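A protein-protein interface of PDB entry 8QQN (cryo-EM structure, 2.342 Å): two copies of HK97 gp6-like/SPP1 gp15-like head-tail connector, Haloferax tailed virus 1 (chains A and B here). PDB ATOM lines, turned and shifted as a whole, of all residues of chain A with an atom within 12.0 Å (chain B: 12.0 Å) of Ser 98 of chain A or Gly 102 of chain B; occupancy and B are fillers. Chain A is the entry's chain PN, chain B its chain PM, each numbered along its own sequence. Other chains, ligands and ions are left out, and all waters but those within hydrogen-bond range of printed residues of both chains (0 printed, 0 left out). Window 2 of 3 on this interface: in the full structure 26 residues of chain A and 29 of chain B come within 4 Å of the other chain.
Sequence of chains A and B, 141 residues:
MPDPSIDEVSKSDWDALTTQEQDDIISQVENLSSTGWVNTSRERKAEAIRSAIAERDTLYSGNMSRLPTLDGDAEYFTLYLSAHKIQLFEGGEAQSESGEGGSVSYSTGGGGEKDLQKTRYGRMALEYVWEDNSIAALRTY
The backbone carbonyl oxygen (O) of Ser 103 of chain B sits at hydrogen-bond distance from the backbone NH (N) of Ser 98 of chain A (2.8 Å). The backbone carbonyl oxygen (O) of Ser 105 of chain B sits at hydrogen-bond distance from the backbone NH (N) of Gln 95 of chain A (2.7 Å). N of Ser 105 of chain B sits at hydrogen-bond distance from O of Ser 96 of chain A, 2.9 Å away.
The backbone NH (N) of Tyr 106 of chain B sits at hydrogen-bond distance from the backbone carbonyl oxygen (O) of Gln 95 of chain B, at 2.8 Å. OG of Ser 105 of chain B sits at hydrogen-bond distance from OG of Ser 96 of chain B. The backbone carbonyl oxygen (O) of Glu 97 of chain B lies within hydrogen-bond range of the backbone NH (N) of Val 104 of chain B (2.9 Å). OG of Ser 96 of chain A sits at hydrogen-bond distance from OG of Ser 105 of chain A. The backbone carbonyl oxygen of Glu 97 of chain A is in hydrogen-bond range of the backbone NH of Val 104 of chain A. The side-chain hydroxyl of Tyr 106 of chain A is in hydrogen-bond range of the side-chain carboxylate of Glu 97 of chain A (2.7 Å).
Among the printed residues, merely in contact across the chains: Glu 93 of chain A with Tyr 106 of chain B (3.4 Å), Ala 94 of chain A with Ser 105 of chain B (3.6 Å), Ser 96 of chain A with Val 104 of chain B (3.3 Å), Glu 97 of chain A with Ser 103 of chain B (3.5 Å) and Ser 98 of chain A with Gly 102 of chain B (3.4 Å).
Ser 98 of chain A touches just these residues of chain B: Gly 102 (3.4 Å) and Ser 103 (2.8 Å). Of chain A, only Ser 98 comes within 4 Å of Gly 102 of chain B. Of chain B, only Val 104 (3.3 Å) and Ser 105 (2.9 Å) come within 4 Å of Ser 96 of chain A. Gly 101 of chain A touches none of the printed residues of chain B. No residue of chain B comes within 4 Å of Gly 102 of chain A. No residue of chain B comes within 4 Å of Ser 103 of chain A. No residue of chain A comes within 4 Å of Ser 98 of chain B. Gly 99 of chain B touches none of the printed residues of chain A. Of chain A, only Glu 97 (3.5 Å) and Ser 98 (2.8 Å) come within 4 Å of Ser 103 of chain B. Val 104 of chain B touches one residue of chain A. Of the printed residues of chain B, Glu 93 of chain A touches Tyr 106. Printed residues of chain A within 4 Å of Ser 105 of chain B: Ala 94, Gln 95 and Ser 96. Printed residues of chain B within 4 Å of Gln 95 of chain A: Ser 105 (2.7 Å). Printed residues of chain A within 4 Å of Tyr 106 of chain B: Glu 93 (3.4 Å). Of the printed residues of chain B, Ala 94 of chain A touches Ser 105. Ser 96 of chain B touches none of the printed residues of chain A. Ser 105 of chain A touches none of the printed residues of chain B. The nearest residue of chain B that does not touch Ser 98 of chain A is Gly 101 of chain B (4.1 Å). The nearest residue of chain A that does not touch Gly 102 of chain B is Gly 99 of chain A (4.6 Å). The nearest printed residue of chain B that does not touch Gln 95 of chain A is Tyr 106 of chain B (4.2 Å).
Printed residues of chain A that touch a printed residue of chain B: Glu 93, Ala 94, Gln 95, Ser 96, Glu 97 and Ser 98. Hydrophobic or aromatic side chains of chain B that line the printed part of chain A: Val 104 and Tyr 106.
Ala 94 of chain A touches Ser 105 of chain B, but with the chains exchanged Ser 105 of chain A does not touch Ala 94 of chain B (15.2 Å). Gln 95 of chain A touches Ser 105 of chain B, but with the chains exchanged Ser 105 of chain A does not touch Gln 95 of chain B (11.5 Å). Ser 96 of chain A touches Ser 105 of chain B, but with the chains exchanged Ser 105 of chain A does not touch Ser 96 of chain B (10.7 Å). Ser 98 of chain A touches Gly 102 of chain B, but with the chains exchanged Gly 102 of chain A does not touch Ser 98 of chain B (11.4 Å). Positions printed for both chains: 94, 95, 96, 97, 98, 99, 100, 101, 102, 103, 104, 105 and 106.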
ATOM      1  N   GLU A  93       5.971  -4.943  -0.738  1.00  0.00           N
ATOM      2  CA  GLU A  93       5.427  -4.954  -2.090  1.00  0.00           C
ATOM      3  C   GLU A  93       6.549  -5.151  -3.116  1.00  0.00           C
ATOM      4  O   GLU A  93       7.562  -4.448  -3.079  1.00  0.00           O
ATOM      5  CB  GLU A  93       4.662  -3.645  -2.285  1.00  0.00           C
ATOM      6  CG  GLU A  93       3.998  -3.468  -3.635  1.00  0.00           C
ATOM      7  CD  GLU A  93       2.656  -2.772  -3.481  1.00  0.00           C
ATOM      8  OE1 GLU A  93       1.689  -3.457  -3.069  1.00  0.00           O
ATOM      9  OE2 GLU A  93       2.583  -1.537  -3.693  1.00  0.00           O
ATOM     10  N   ALA A  94       6.346  -6.085  -4.059  1.00  0.00           N
ATOM     11  CA  ALA A  94       7.304  -6.324  -5.131  1.00  0.00           C
ATOM     12  C   ALA A  94       7.258  -5.190  -6.160  1.00  0.00           C
ATOM     13  O   ALA A  94       6.189  -4.755  -6.600  1.00  0.00           O
ATOM     14  CB  ALA A  94       7.075  -7.684  -5.761  1.00  0.00           C
ATOM     15  N   GLN A  95       8.448  -4.717  -6.546  1.00  0.00           N
ATOM     16  CA  GLN A  95       8.606  -3.736  -7.605  1.00  0.00           C
ATOM     17  C   GLN A  95       8.974  -4.441  -8.913  1.00  0.00           C
ATOM     18  O   GLN A  95       8.382  -4.157  -9.950  1.00  0.00           O
ATOM     19  CB  GLN A  95       9.626  -2.694  -7.159  1.00  0.00           C
ATOM     20  CG  GLN A  95       9.861  -1.590  -8.180  1.00  0.00           C
ATOM     21  CD  GLN A  95      10.747  -0.477  -7.670  1.00  0.00           C
ATOM     22  OE1 GLN A  95      11.366  -0.575  -6.610  1.00  0.00           O
ATOM     23  NE2 GLN A  95      10.823   0.608  -8.431  1.00  0.00           N
ATOM     24  N   SER A  96       9.946  -5.362  -8.852  1.00  0.00           N
ATOM     25  CA  SER A  96      10.339  -6.183  -9.990  1.00  0.00           C
ATOM     26  C   SER A  96      10.471  -7.639  -9.556  1.00  0.00           C
ATOM     27  O   SER A  96      10.979  -7.926  -8.473  1.00  0.00           O
ATOM     28  CB  SER A  96      11.627  -5.706 -10.613  1.00  0.00           C
ATOM     29  OG  SER A  96      11.519  -4.376 -11.086  1.00  0.00           O
ATOM     30  N   GLU A  97      10.029  -8.544 -10.437  1.00  0.00           N
ATOM     31  CA  GLU A  97      10.193  -9.984 -10.284  1.00  0.00           C
ATOM     32  C   GLU A  97      10.794 -10.548 -11.576  1.00  0.00           C
ATOM     33  O   GLU A  97      10.252 -10.314 -12.658  1.00  0.00           O
ATOM     34  CB  GLU A  97       8.843 -10.645  -9.978  1.00  0.00           C
ATOM     35  CG  GLU A  97       8.160 -10.150  -8.706  1.00  0.00           C
ATOM     36  CD  GLU A  97       6.760 -10.707  -8.490  1.00  0.00           C
ATOM     37  OE1 GLU A  97       5.895 -10.527  -9.374  1.00  0.00           O
ATOM     38  OE2 GLU A  97       6.541 -11.338  -7.437  1.00  0.00           O
ATOM     39  N   SER A  98      11.912 -11.289 -11.462  1.00  0.00           N
ATOM     40  CA  SER A  98      12.551 -11.968 -12.586  1.00  0.00           C
ATOM     41  C   SER A  98      12.790 -13.440 -12.259  1.00  0.00           C
ATOM     42  O   SER A  98      13.254 -13.769 -11.170  1.00  0.00           O
ATOM     43  CB  SER A  98      13.856 -11.322 -12.976  1.00  0.00           C
ATOM     44  OG  SER A  98      13.668 -10.000 -13.445  1.00  0.00           O
ATOM     45  N   GLY A  99      12.507 -14.310 -13.235  1.00  0.00           N
ATOM     46  CA  GLY A  99      12.618 -15.750 -13.074  1.00  0.00           C
ATOM     47  C   GLY A  99      13.430 -16.380 -14.199  1.00  0.00           C
ATOM     48  O   GLY A  99      14.505 -15.888 -14.532  1.00  0.00           O
ATOM     49  N   GLU A 100      12.887 -17.455 -14.785  1.00  0.00           N
ATOM     50  CA  GLU A 100      13.514 -18.172 -15.886  1.00  0.00           C
ATOM     51  C   GLU A 100      13.319 -17.377 -17.184  1.00  0.00           C
ATOM     52  O   GLU A 100      12.473 -17.711 -18.017  1.00  0.00           O
ATOM     53  CB  GLU A 100      13.010 -19.621 -15.912  1.00  0.00           C
ATOM     54  CG  GLU A 100      13.723 -20.523 -16.913  1.00  0.00           C
ATOM     55  CD  GLU A 100      15.238 -20.628 -16.805  1.00  0.00           C
ATOM     56  OE1 GLU A 100      15.761 -20.592 -15.669  1.00  0.00           O
ATOM     57  OE2 GLU A 100      15.893 -20.749 -17.862  1.00  0.00           O
ATOM     58  N   GLY A 101      14.114 -16.307 -17.340  1.00  0.00           N
ATOM     59  CA  GLY A 101      14.008 -15.384 -18.464  1.00  0.00           C
ATOM     60  C   GLY A 101      12.898 -14.339 -18.297  1.00  0.00           C
ATOM     61  O   GLY A 101      13.095 -13.162 -18.617  1.00  0.00           O
ATOM     62  N   GLY A 102      11.727 -14.766 -17.795  1.00  0.00           N
ATOM     63  CA  GLY A 102      10.558 -13.905 -17.640  1.00  0.00           C
ATOM     64  C   GLY A 102      10.759 -12.816 -16.584  1.00  0.00           C
ATOM     65  O   GLY A 102      11.243 -13.100 -15.490  1.00  0.00           O
ATOM     66  N   SER A 103      10.382 -11.571 -16.920  1.00  0.00           N
ATOM     67  CA  SER A 103      10.474 -10.436 -16.006  1.00  0.00           C
ATOM     68  C   SER A 103       9.227  -9.557 -16.058  1.00  0.00           C
ATOM     69  O   SER A 103       8.652  -9.323 -17.120  1.00  0.00           O
ATOM     70  CB  SER A 103      11.695  -9.594 -16.267  1.00  0.00           C
ATOM     71  OG  SER A 103      12.887 -10.338 -16.076  1.00  0.00           O
ATOM     72  N   VAL A 104       8.846  -9.026 -14.891  1.00  0.00           N
ATOM     73  CA  VAL A 104       7.809  -8.011 -14.789  1.00  0.00           C
ATOM     74  C   VAL A 104       8.265  -6.920 -13.814  1.00  0.00           C
ATOM     75  O   VAL A 104       8.915  -7.203 -12.807  1.00  0.00           O
ATOM     76  CB  VAL A 104       6.439  -8.627 -14.425  1.00  0.00           C
ATOM     77  CG1 VAL A 104       6.466  -9.398 -13.115  1.00  0.00           C
ATOM     78  CG2 VAL A 104       5.317  -7.601 -14.401  1.00  0.00           C
ATOM     79  N   SER A 105       7.934  -5.663 -14.145  1.00  0.00           N
ATOM     80  CA  SER A 105       8.067  -4.519 -13.251  1.00  0.00           C
ATOM     81  C   SER A 105       6.695  -3.886 -13.051  1.00  0.00           C
ATOM     82  O   SER A 105       5.919  -3.786 -13.999  1.00  0.00           O
ATOM     83  CB  SER A 105       9.044  -3.501 -13.781  1.00  0.00           C
ATOM     84  OG  SER A 105      10.372  -3.980 -13.651  1.00  0.00           O
ATOM     85  N   TYR A 106       6.426  -3.420 -11.825  1.00  0.00           N
ATOM     86  CA  TYR A 106       5.136  -2.853 -11.464  1.00  0.00           C
ATOM     87  C   TYR A 106       5.248  -1.361 -11.145  1.00  0.00           C
ATOM     88  O   TYR A 106       6.274  -0.876 -10.669  1.00  0.00           O
ATOM     89  CB  TYR A 106       4.524  -3.602 -10.281  1.00  0.00           C
ATOM     90  CG  TYR A 106       4.386  -5.095 -10.435  1.00  0.00           C
ATOM     91  CD1 TYR A 106       3.308  -5.659 -11.104  1.00  0.00           C
ATOM     92  CD2 TYR A 106       5.314  -5.954  -9.864  1.00  0.00           C
ATOM     93  CE1 TYR A 106       3.177  -7.037 -11.233  1.00  0.00           C
ATOM     94  CE2 TYR A 106       5.192  -7.332  -9.972  1.00  0.00           C
ATOM     95  CZ  TYR A 106       4.116  -7.877 -10.656  1.00  0.00           C
ATOM     96  OH  TYR A 106       3.984  -9.235 -10.753  1.00  0.00           O
ATOM     97  N   ALA B  94      15.909  -5.957   3.326  1.00  0.00           N
ATOM     98  CA  ALA B  94      16.375  -6.261   1.980  1.00  0.00           C
ATOM     99  C   ALA B  94      15.589  -5.445   0.952  1.00  0.00           C
ATOM    100  O   ALA B  94      14.357  -5.430   0.957  1.00  0.00           O
ATOM    101  CB  ALA B  94      16.286  -7.746   1.717  1.00  0.00           C
ATOM    102  N   GLN B  95      16.327  -4.787   0.048  1.00  0.00           N
ATOM    103  CA  GLN B  95      15.772  -4.022  -1.058  1.00  0.00           C
ATOM    104  C   GLN B  95      15.728  -4.883  -2.325  1.00  0.00           C
ATOM    105  O   GLN B  95      14.731  -4.866  -3.045  1.00  0.00           O
ATOM    106  CB  GLN B  95      16.606  -2.754  -1.208  1.00  0.00           C
ATOM    107  CG  GLN B  95      16.191  -1.854  -2.365  1.00  0.00           C
ATOM    108  CD  GLN B  95      16.949  -0.546  -2.408  1.00  0.00           C
ATOM    109  OE1 GLN B  95      17.954  -0.357  -1.721  1.00  0.00           O
ATOM    110  NE2 GLN B  95      16.473   0.380  -3.231  1.00  0.00           N
ATOM    111  N   SER B  96      16.808  -5.631  -2.590  1.00  0.00           N
ATOM    112  CA  SER B  96      16.884  -6.575  -3.698  1.00  0.00           C
ATOM    113  C   SER B  96      17.497  -7.885  -3.215  1.00  0.00           C
ATOM    114  O   SER B  96      18.425  -7.881  -2.408  1.00  0.00           O
ATOM    115  CB  SER B  96      17.685  -6.029  -4.854  1.00  0.00           C
ATOM    116  OG  SER B  96      17.097  -4.861  -5.395  1.00  0.00           O
ATOM    117  N   GLU B  97      16.978  -8.995  -3.749  1.00  0.00           N
ATOM    118  CA  GLU B  97      17.519 -10.332  -3.543  1.00  0.00           C
ATOM    119  C   GLU B  97      17.650 -11.015  -4.907  1.00  0.00           C
ATOM    120  O   GLU B  97      16.692 -11.036  -5.681  1.00  0.00           O
ATOM    121  CB  GLU B  97      16.604 -11.138  -2.614  1.00  0.00           C
ATOM    122  CG  GLU B  97      16.443 -10.554  -1.216  1.00  0.00           C
ATOM    123  CD  GLU B  97      15.421 -11.272  -0.345  1.00  0.00           C
ATOM    124  OE1 GLU B  97      14.244 -11.375  -0.755  1.00  0.00           O
ATOM    125  OE2 GLU B  97      15.809 -11.742   0.745  1.00  0.00           O
ATOM    126  N   SER B  98      18.843 -11.560  -5.202  1.00  0.00           N
ATOM    127  CA  SER B  98      19.107 -12.323  -6.417  1.00  0.00           C
ATOM    128  C   SER B  98      19.782 -13.644  -6.057  1.00  0.00           C
ATOM    129  O   SER B  98      20.707 -13.667  -5.249  1.00  0.00           O
ATOM    130  CB  SER B  98      19.973 -11.562  -7.391  1.00  0.00           C
ATOM    131  OG  SER B  98      19.316 -10.413  -7.898  1.00  0.00           O
ATOM    132  N   GLY B  99      19.330 -14.729  -6.691  1.00  0.00           N
ATOM    133  CA  GLY B  99      19.814 -16.070  -6.406  1.00  0.00           C
ATOM    134  C   GLY B  99      20.209 -16.803  -7.680  1.00  0.00           C
ATOM    135  O   GLY B  99      20.841 -16.218  -8.554  1.00  0.00           O
ATOM    136  N   GLU B 100      19.800 -18.075  -7.777  1.00  0.00           N
ATOM    137  CA  GLU B 100      20.020 -18.901  -8.955  1.00  0.00           C
ATOM    138  C   GLU B 100      19.065 -18.457 -10.070  1.00  0.00           C
ATOM    139  O   GLU B 100      18.039 -19.093 -10.324  1.00  0.00           O
ATOM    140  CB  GLU B 100      19.931 -20.383  -8.574  1.00  0.00           C
ATOM    141  CG  GLU B 100      20.347 -21.340  -9.685  1.00  0.00           C
ATOM    142  CD  GLU B 100      21.766 -21.201 -10.219  1.00  0.00           C
ATOM    143  OE1 GLU B 100      22.665 -20.818  -9.438  1.00  0.00           O
ATOM    144  OE2 GLU B 100      21.969 -21.471 -11.421  1.00  0.00           O
ATOM    145  N   GLY B 101      19.416 -17.344 -10.733  1.00  0.00           N
ATOM    146  CA  GLY B 101      18.602 -16.740 -11.781  1.00  0.00           C
ATOM    147  C   GLY B 101      17.465 -15.860 -11.249  1.00  0.00           C
ATOM    148  O   GLY B 101      17.209 -14.779 -11.789  1.00  0.00           O
ATOM    149  N   GLY B 102      16.770 -16.321 -10.197  1.00  0.00           N
ATOM    150  CA  GLY B 102      15.635 -15.607  -9.621  1.00  0.00           C
ATOM    151  C   GLY B 102      16.042 -14.274  -8.987  1.00  0.00           C
ATOM    152  O   GLY B 102      17.057 -14.205  -8.298  1.00  0.00           O
ATOM    153  N   SER B 103      15.260 -13.213  -9.244  1.00  0.00           N
ATOM    154  CA  SER B 103      15.477 -11.907  -8.629  1.00  0.00           C
ATOM    155  C   SER B 103      14.164 -11.250  -8.214  1.00  0.00           C
ATOM    156  O   SER B 103      13.163 -11.315  -8.927  1.00  0.00           O
ATOM    157  CB  SER B 103      16.246 -10.973  -9.524  1.00  0.00           C
ATOM    158  OG  SER B 103      17.560 -11.448  -9.760  1.00  0.00           O
ATOM    159  N   VAL B 104      14.197 -10.566  -7.064  1.00  0.00           N
ATOM    160  CA  VAL B 104      13.097  -9.724  -6.619  1.00  0.00           C
ATOM    161  C   VAL B 104      13.652  -8.398  -6.087  1.00  0.00           C
ATOM    162  O   VAL B 104      14.700  -8.363  -5.440  1.00  0.00           O
ATOM    163  CB  VAL B 104      12.186 -10.456  -5.607  1.00  0.00           C
ATOM    164  CG1 VAL B 104      12.936 -10.941  -4.377  1.00  0.00           C
ATOM    165  CG2 VAL B 104      10.990  -9.619  -5.189  1.00  0.00           C
ATOM    166  N   SER B 105      12.938  -7.301  -6.386  1.00  0.00           N
ATOM    167  CA  SER B 105      13.157  -5.995  -5.775  1.00  0.00           C
ATOM    168  C   SER B 105      11.885  -5.561  -5.055  1.00  0.00           C
ATOM    169  O   SER B 105      10.791  -5.740  -5.582  1.00  0.00           O
ATOM    170  CB  SER B 105      13.561  -4.961  -6.792  1.00  0.00           C
ATOM    171  OG  SER B 105      14.891  -5.195  -7.223  1.00  0.00           O
ATOM    172  N   TYR B 106      12.041  -4.944  -3.877  1.00  0.00           N
ATOM    173  CA  TYR B 106      10.912  -4.517  -3.065  1.00  0.00           C
ATOM    174  C   TYR B 106      10.836  -2.995  -2.963  1.00  0.00           C
ATOM    175  O   TYR B 106      11.849  -2.311  -2.824  1.00  0.00           O
ATOM    176  CB  TYR B 106      11.026  -5.091  -1.654  1.00  0.00           C
ATOM    177  CG  TYR B 106      11.202  -6.583  -1.552  1.00  0.00           C
ATOM    178  CD1 TYR B 106      10.107  -7.436  -1.547  1.00  0.00           C
ATOM    179  CD2 TYR B 106      12.463  -7.140  -1.395  1.00  0.00           C
ATOM    180  CE1 TYR B 106      10.265  -8.810  -1.425  1.00  0.00           C
ATOM    181  CE2 TYR B 106      12.638  -8.511  -1.265  1.00  0.00           C
ATOM    182  CZ  TYR B 106      11.533  -9.350  -1.272  1.00  0.00           C
ATOM    183  OH  TYR B 106      11.690 -10.700  -1.122  1.00  0.00           O
